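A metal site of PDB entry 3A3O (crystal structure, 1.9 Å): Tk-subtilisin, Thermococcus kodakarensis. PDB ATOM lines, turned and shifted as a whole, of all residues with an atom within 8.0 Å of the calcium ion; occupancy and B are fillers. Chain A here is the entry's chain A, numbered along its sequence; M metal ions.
The side-chain amide nitrogen of Gln 15 is in hydrogen-bond range of the side-chain amide oxygen of Asn 96. N of Gln 15 lies within hydrogen-bond range of O of Asp 98.
The calcium ion is bound by the backbone carbonyl oxygen (O) of Leu 95, the backbone carbonyl oxygen (O) of Val 101, the backbone carbonyl oxygen (O) of Ile 99, the side-chain amide oxygen (OD1) of Asn 97, the side-chain amide oxygen (OE1) of Gln 15, the side-chain carboxylate (OD1) of Asp 55 and the side-chain carboxylate (OD2) of Asp 55.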
ATOM      1  N   GLN A  12      19.353 -26.661  -7.065  1.00  0.00           N
ATOM      2  CA  GLN A  12      20.071 -26.059  -5.876  1.00  0.00           C
ATOM      3  C   GLN A  12      19.686 -26.780  -4.586  1.00  0.00           C
ATOM      4  O   GLN A  12      18.501 -26.909  -4.290  1.00  0.00           O
ATOM      5  CB  GLN A  12      19.769 -24.562  -5.737  1.00  0.00           C
ATOM      6  CG  GLN A  12      20.459 -23.660  -6.765  1.00  0.00           C
ATOM      7  CD  GLN A  12      21.980 -23.623  -6.599  1.00  0.00           C
ATOM      8  OE1 GLN A  12      22.499 -23.629  -5.483  1.00  0.00           O
ATOM      9  NE2 GLN A  12      22.704 -23.625  -7.710  1.00  0.00           N
ATOM     10  N   PRO A  13      20.686 -27.219  -3.790  1.00  0.00           N
ATOM     11  CA  PRO A  13      20.364 -27.856  -2.512  1.00  0.00           C
ATOM     12  C   PRO A  13      19.849 -26.875  -1.464  1.00  0.00           C
ATOM     13  O   PRO A  13      20.141 -25.664  -1.558  1.00  0.00           O
ATOM     14  CB  PRO A  13      21.706 -28.445  -2.055  1.00  0.00           C
ATOM     15  CG  PRO A  13      22.765 -27.580  -2.752  1.00  0.00           C
ATOM     16  CD  PRO A  13      22.137 -27.118  -4.054  1.00  0.00           C
ATOM     17  N   ALA A  14      19.099 -27.390  -0.471  1.00  0.00           N
ATOM     18  CA  ALA A  14      18.652 -26.619   0.696  1.00  0.00           C
ATOM     19  C   ALA A  14      19.854 -26.118   1.493  1.00  0.00           C
ATOM     20  O   ALA A  14      20.890 -26.810   1.559  1.00  0.00           O
ATOM     21  CB  ALA A  14      17.740 -27.464   1.583  1.00  0.00           C
ATOM     22  N   GLN A  15      19.708 -24.932   2.089  1.00  0.00           N
ATOM     23  CA  GLN A  15      20.820 -24.275   2.803  1.00  0.00           C
ATOM     24  C   GLN A  15      21.293 -25.051   4.032  1.00  0.00           C
ATOM     25  O   GLN A  15      20.479 -25.523   4.835  1.00  0.00           O
ATOM     26  CB  GLN A  15      20.447 -22.846   3.217  1.00  0.00           C
ATOM     27  CG  GLN A  15      21.586 -22.057   3.881  1.00  0.00           C
ATOM     28  CD  GLN A  15      21.287 -20.599   4.034  1.00  0.00           C
ATOM     29  OE1 GLN A  15      21.402 -19.838   3.070  1.00  0.00           O
ATOM     30  NE2 GLN A  15      20.881 -20.191   5.238  1.00  0.00           N
ATOM     31  N   THR A  16      22.623 -25.208   4.160  1.00  0.00           N
ATOM     32  CA  THR A  16      23.223 -25.599   5.441  1.00  0.00           C
ATOM     33  C   THR A  16      24.141 -24.518   5.914  1.00  0.00           C
ATOM     34  O   THR A  16      24.652 -23.747   5.102  1.00  0.00           O
ATOM     35  CB  THR A  16      24.263 -26.727   5.340  1.00  0.00           C
ATOM     36  OG1 THR A  16      24.487 -27.116   3.974  1.00  0.00           O
ATOM     37  CG2 THR A  16      23.977 -27.859   6.305  1.00  0.00           C
ATOM     38  N   HIS A  53      26.566 -17.022  -9.670  1.00  0.00           N
ATOM     39  CA  HIS A  53      26.168 -18.067  -8.733  1.00  0.00           C
ATOM     40  C   HIS A  53      24.951 -17.607  -7.932  1.00  0.00           C
ATOM     41  O   HIS A  53      24.943 -16.503  -7.388  1.00  0.00           O
ATOM     42  CB  HIS A  53      27.329 -18.437  -7.806  1.00  0.00           C
ATOM     43  CG  HIS A  53      27.073 -19.670  -6.995  1.00  0.00           C
ATOM     44  ND1 HIS A  53      27.892 -20.769  -7.045  1.00  0.00           N
ATOM     45  CD2 HIS A  53      26.083 -19.972  -6.128  1.00  0.00           C
ATOM     46  CE1 HIS A  53      27.438 -21.696  -6.218  1.00  0.00           C
ATOM     47  NE2 HIS A  53      26.326 -21.247  -5.662  1.00  0.00           N
ATOM     48  N   PRO A  54      23.869 -18.410  -7.887  1.00  0.00           N
ATOM     49  CA  PRO A  54      22.654 -17.972  -7.154  1.00  0.00           C
ATOM     50  C   PRO A  54      22.890 -17.695  -5.669  1.00  0.00           C
ATOM     51  O   PRO A  54      22.132 -16.937  -5.031  1.00  0.00           O
ATOM     52  CB  PRO A  54      21.688 -19.165  -7.300  1.00  0.00           C
ATOM     53  CG  PRO A  54      22.154 -19.896  -8.517  1.00  0.00           C
ATOM     54  CD  PRO A  54      23.676 -19.721  -8.554  1.00  0.00           C
ATOM     55  N   ASP A  55      23.925 -18.298  -5.094  1.00  0.00           N
ATOM     56  CA  ASP A  55      24.212 -18.055  -3.666  1.00  0.00           C
ATOM     57  C   ASP A  55      25.249 -16.962  -3.412  1.00  0.00           C
ATOM     58  O   ASP A  55      25.662 -16.758  -2.259  1.00  0.00           O
ATOM     59  CB  ASP A  55      24.594 -19.345  -2.918  1.00  0.00           C
ATOM     60  CG  ASP A  55      23.949 -19.405  -1.533  1.00  0.00           C
ATOM     61  OD1 ASP A  55      22.908 -18.744  -1.307  1.00  0.00           O
ATOM     62  OD2 ASP A  55      24.439 -20.118  -0.638  1.00  0.00           O
ATOM     63  N   LEU A  56      25.649 -16.268  -4.496  1.00  0.00           N
ATOM     64  CA  LEU A  56      26.640 -15.183  -4.430  1.00  0.00           C
ATOM     65  C   LEU A  56      26.219 -13.887  -5.101  1.00  0.00           C
ATOM     66  O   LEU A  56      26.652 -12.786  -4.703  1.00  0.00           O
ATOM     67  CB  LEU A  56      27.956 -15.626  -5.078  1.00  0.00           C
ATOM     68  CG  LEU A  56      28.799 -16.768  -4.481  1.00  0.00           C
ATOM     69  CD1 LEU A  56      30.082 -16.835  -5.269  1.00  0.00           C
ATOM     70  CD2 LEU A  56      29.103 -16.541  -3.013  1.00  0.00           C
ATOM     71  N   ALA A  93      30.707 -14.516   2.196  1.00  0.00           N
ATOM     72  CA  ALA A  93      29.512 -13.737   1.791  1.00  0.00           C
ATOM     73  C   ALA A  93      28.411 -14.515   1.091  1.00  0.00           C
ATOM     74  O   ALA A  93      27.515 -13.892   0.468  1.00  0.00           O
ATOM     75  CB  ALA A  93      29.944 -12.581   0.922  1.00  0.00           C
ATOM     76  N   ALA A  94      28.442 -15.856   1.186  1.00  0.00           N
ATOM     77  CA  ALA A  94      27.305 -16.627   0.627  1.00  0.00           C
ATOM     78  C   ALA A  94      25.999 -16.142   1.290  1.00  0.00           C
ATOM     79  O   ALA A  94      25.965 -15.880   2.493  1.00  0.00           O
ATOM     80  CB  ALA A  94      27.496 -18.116   0.834  1.00  0.00           C
ATOM     81  N   LEU A  95      24.931 -16.011   0.502  1.00  0.00           N
ATOM     82  CA  LEU A  95      23.696 -15.381   0.978  1.00  0.00           C
ATOM     83  C   LEU A  95      22.938 -16.263   1.971  1.00  0.00           C
ATOM     84  O   LEU A  95      22.940 -17.506   1.853  1.00  0.00           O
ATOM     85  CB  LEU A  95      22.817 -15.067  -0.244  1.00  0.00           C
ATOM     86  CG  LEU A  95      23.387 -13.996  -1.178  1.00  0.00           C
ATOM     87  CD1 LEU A  95      22.965 -14.206  -2.662  1.00  0.00           C
ATOM     88  CD2 LEU A  95      22.980 -12.604  -0.702  1.00  0.00           C
ATOM     89  N   ASN A  96      22.301 -15.620   2.944  1.00  0.00           N
ATOM     90  CA  ASN A  96      21.453 -16.316   3.908  1.00  0.00           C
ATOM     91  C   ASN A  96      20.046 -16.398   3.301  1.00  0.00           C
ATOM     92  O   ASN A  96      19.324 -15.404   3.260  1.00  0.00           O
ATOM     93  CB  ASN A  96      21.417 -15.556   5.216  1.00  0.00           C
ATOM     94  CG  ASN A  96      20.725 -16.331   6.330  1.00  0.00           C
ATOM     95  OD1 ASN A  96      20.306 -17.470   6.126  1.00  0.00           O
ATOM     96  ND2 ASN A  96      20.607 -15.721   7.496  1.00  0.00           N
ATOM     97  N   ASN A  97      19.691 -17.575   2.797  1.00  0.00           N
ATOM     98  CA  ASN A  97      18.456 -17.752   2.028  1.00  0.00           C
ATOM     99  C   ASN A  97      18.023 -19.215   2.125  1.00  0.00           C
ATOM    100  O   ASN A  97      18.356 -19.891   3.093  1.00  0.00           O
ATOM    101  CB  ASN A  97      18.669 -17.283   0.553  1.00  0.00           C
ATOM    102  CG  ASN A  97      19.870 -17.968  -0.144  1.00  0.00           C
ATOM    103  OD1 ASN A  97      20.410 -18.971   0.337  1.00  0.00           O
ATOM    104  ND2 ASN A  97      20.262 -17.441  -1.313  1.00  0.00           N
ATOM    105  N   ASP A  98      17.360 -19.722   1.094  1.00  0.00           N
ATOM    106  CA  ASP A  98      16.866 -21.086   1.142  1.00  0.00           C
ATOM    107  C   ASP A  98      17.785 -22.129   0.532  1.00  0.00           C
ATOM    108  O   ASP A  98      17.445 -23.303   0.517  1.00  0.00           O
ATOM    109  CB  ASP A  98      15.454 -21.162   0.513  1.00  0.00           C
ATOM    110  CG  ASP A  98      14.454 -20.268   1.224  1.00  0.00           C
ATOM    111  OD1 ASP A  98      14.386 -20.308   2.486  1.00  0.00           O
ATOM    112  OD2 ASP A  98      13.721 -19.508   0.534  1.00  0.00           O
ATOM    113  N   ILE A  99      18.948 -21.706   0.040  1.00  0.00           N
ATOM    114  CA  ILE A  99      19.825 -22.580  -0.738  1.00  0.00           C
ATOM    115  C   ILE A  99      21.300 -22.575  -0.309  1.00  0.00           C
ATOM    116  O   ILE A  99      21.785 -21.603   0.258  1.00  0.00           O
ATOM    117  CB  ILE A  99      19.775 -22.238  -2.260  1.00  0.00           C
ATOM    118  CG1 ILE A  99      20.126 -20.752  -2.501  1.00  0.00           C
ATOM    119  CG2 ILE A  99      18.362 -22.563  -2.852  1.00  0.00           C
ATOM    120  CD1 ILE A  99      20.564 -20.457  -3.921  1.00  0.00           C
ATOM    121  N   GLY A 100      21.998 -23.663  -0.590  1.00  0.00           N
ATOM    122  CA  GLY A 100      23.450 -23.656  -0.629  1.00  0.00           C
ATOM    123  C   GLY A 100      24.092 -23.548   0.730  1.00  0.00           C
ATOM    124  O   GLY A 100      23.904 -24.423   1.582  1.00  0.00           O
ATOM    125  N   VAL A 101      24.893 -22.512   0.948  1.00  0.00           N
ATOM    126  CA  VAL A 101      25.586 -22.351   2.228  1.00  0.00           C
ATOM    127  C   VAL A 101      25.290 -20.941   2.749  1.00  0.00           C
ATOM    128  O   VAL A 101      24.328 -20.313   2.295  1.00  0.00           O
ATOM    129  CB  VAL A 101      27.104 -22.662   2.090  1.00  0.00           C
ATOM    130  CG1 VAL A 101      27.341 -24.164   1.834  1.00  0.00           C
ATOM    131  CG2 VAL A 101      27.776 -21.784   0.971  1.00  0.00           C
ATOM    132  N   VAL A 102      26.072 -20.428   3.698  1.00  0.00           N
ATOM    133  CA  VAL A 102      25.904 -19.057   4.174  1.00  0.00           C
ATOM    134  C   VAL A 102      27.278 -18.586   4.653  1.00  0.00           C
ATOM    135  O   VAL A 102      28.000 -19.360   5.259  1.00  0.00           O
ATOM    136  CB  VAL A 102      24.820 -18.940   5.293  1.00  0.00           C
ATOM    137  CG1 VAL A 102      25.166 -19.782   6.549  1.00  0.00           C
ATOM    138  CG2 VAL A 102      24.516 -17.488   5.641  1.00  0.00           C
ATOM    139  N   GLY A 103      27.614 -17.321   4.364  1.00  0.00           N
ATOM    140  CA  GLY A 103      28.937 -16.775   4.719  1.00  0.00           C
ATOM    141  C   GLY A 103      28.932 -16.263   6.145  1.00  0.00           C
ATOM    142  O   GLY A 103      27.885 -16.189   6.799  1.00  0.00           O
ATOM    143  N   PRO A 106      26.871 -12.616   5.562  1.00  0.00           N
ATOM    144  CA  PRO A 106      26.072 -12.949   4.408  1.00  0.00           C
ATOM    145  C   PRO A 106      25.397 -11.775   3.668  1.00  0.00           C
ATOM    146  O   PRO A 106      24.790 -12.024   2.629  1.00  0.00           O
ATOM    147  CB  PRO A 106      25.053 -13.956   4.959  1.00  0.00           C
ATOM    148  CG  PRO A 106      24.948 -13.721   6.379  1.00  0.00           C
ATOM    149  CD  PRO A 106      26.278 -13.110   6.817  1.00  0.00           C
ATOM    150  N   THR A 242      30.714 -22.329  -1.847  1.00  0.00           N
ATOM    151  CA  THR A 242      30.348 -22.203  -3.250  1.00  0.00           C
ATOM    152  C   THR A 242      31.518 -22.630  -4.174  1.00  0.00           C
ATOM    153  O   THR A 242      32.701 -22.509  -3.814  1.00  0.00           O
ATOM    154  CB  THR A 242      29.882 -20.758  -3.555  1.00  0.00           C
ATOM    155  OG1 THR A 242      30.808 -19.839  -2.952  1.00  0.00           O
ATOM    156  CG2 THR A 242      28.479 -20.511  -2.904  1.00  0.00           C
ATOM    157  N   TYR A 248      28.855 -26.435  -5.325  1.00  0.00           N
ATOM    158  CA  TYR A 248      29.444 -26.364  -3.968  1.00  0.00           C
ATOM    159  C   TYR A 248      30.570 -27.383  -3.926  1.00  0.00           C
ATOM    160  O   TYR A 248      30.550 -28.369  -4.687  1.00  0.00           O
ATOM    161  CB  TYR A 248      28.368 -26.595  -2.852  1.00  0.00           C
ATOM    162  CG  TYR A 248      27.238 -25.635  -3.006  1.00  0.00           C
ATOM    163  CD1 TYR A 248      26.177 -25.928  -3.884  1.00  0.00           C
ATOM    164  CD2 TYR A 248      27.274 -24.373  -2.408  1.00  0.00           C
ATOM    165  CE1 TYR A 248      25.182 -25.027  -4.129  1.00  0.00           C
ATOM    166  CE2 TYR A 248      26.272 -23.458  -2.635  1.00  0.00           C
ATOM    167  CZ  TYR A 248      25.223 -23.791  -3.505  1.00  0.00           C
ATOM    168  OH  TYR A 248      24.228 -22.880  -3.752  1.00  0.00           O
HETATM  169 CA    CA M   1      22.592 -19.571   0.990  1.00  0.00          CA
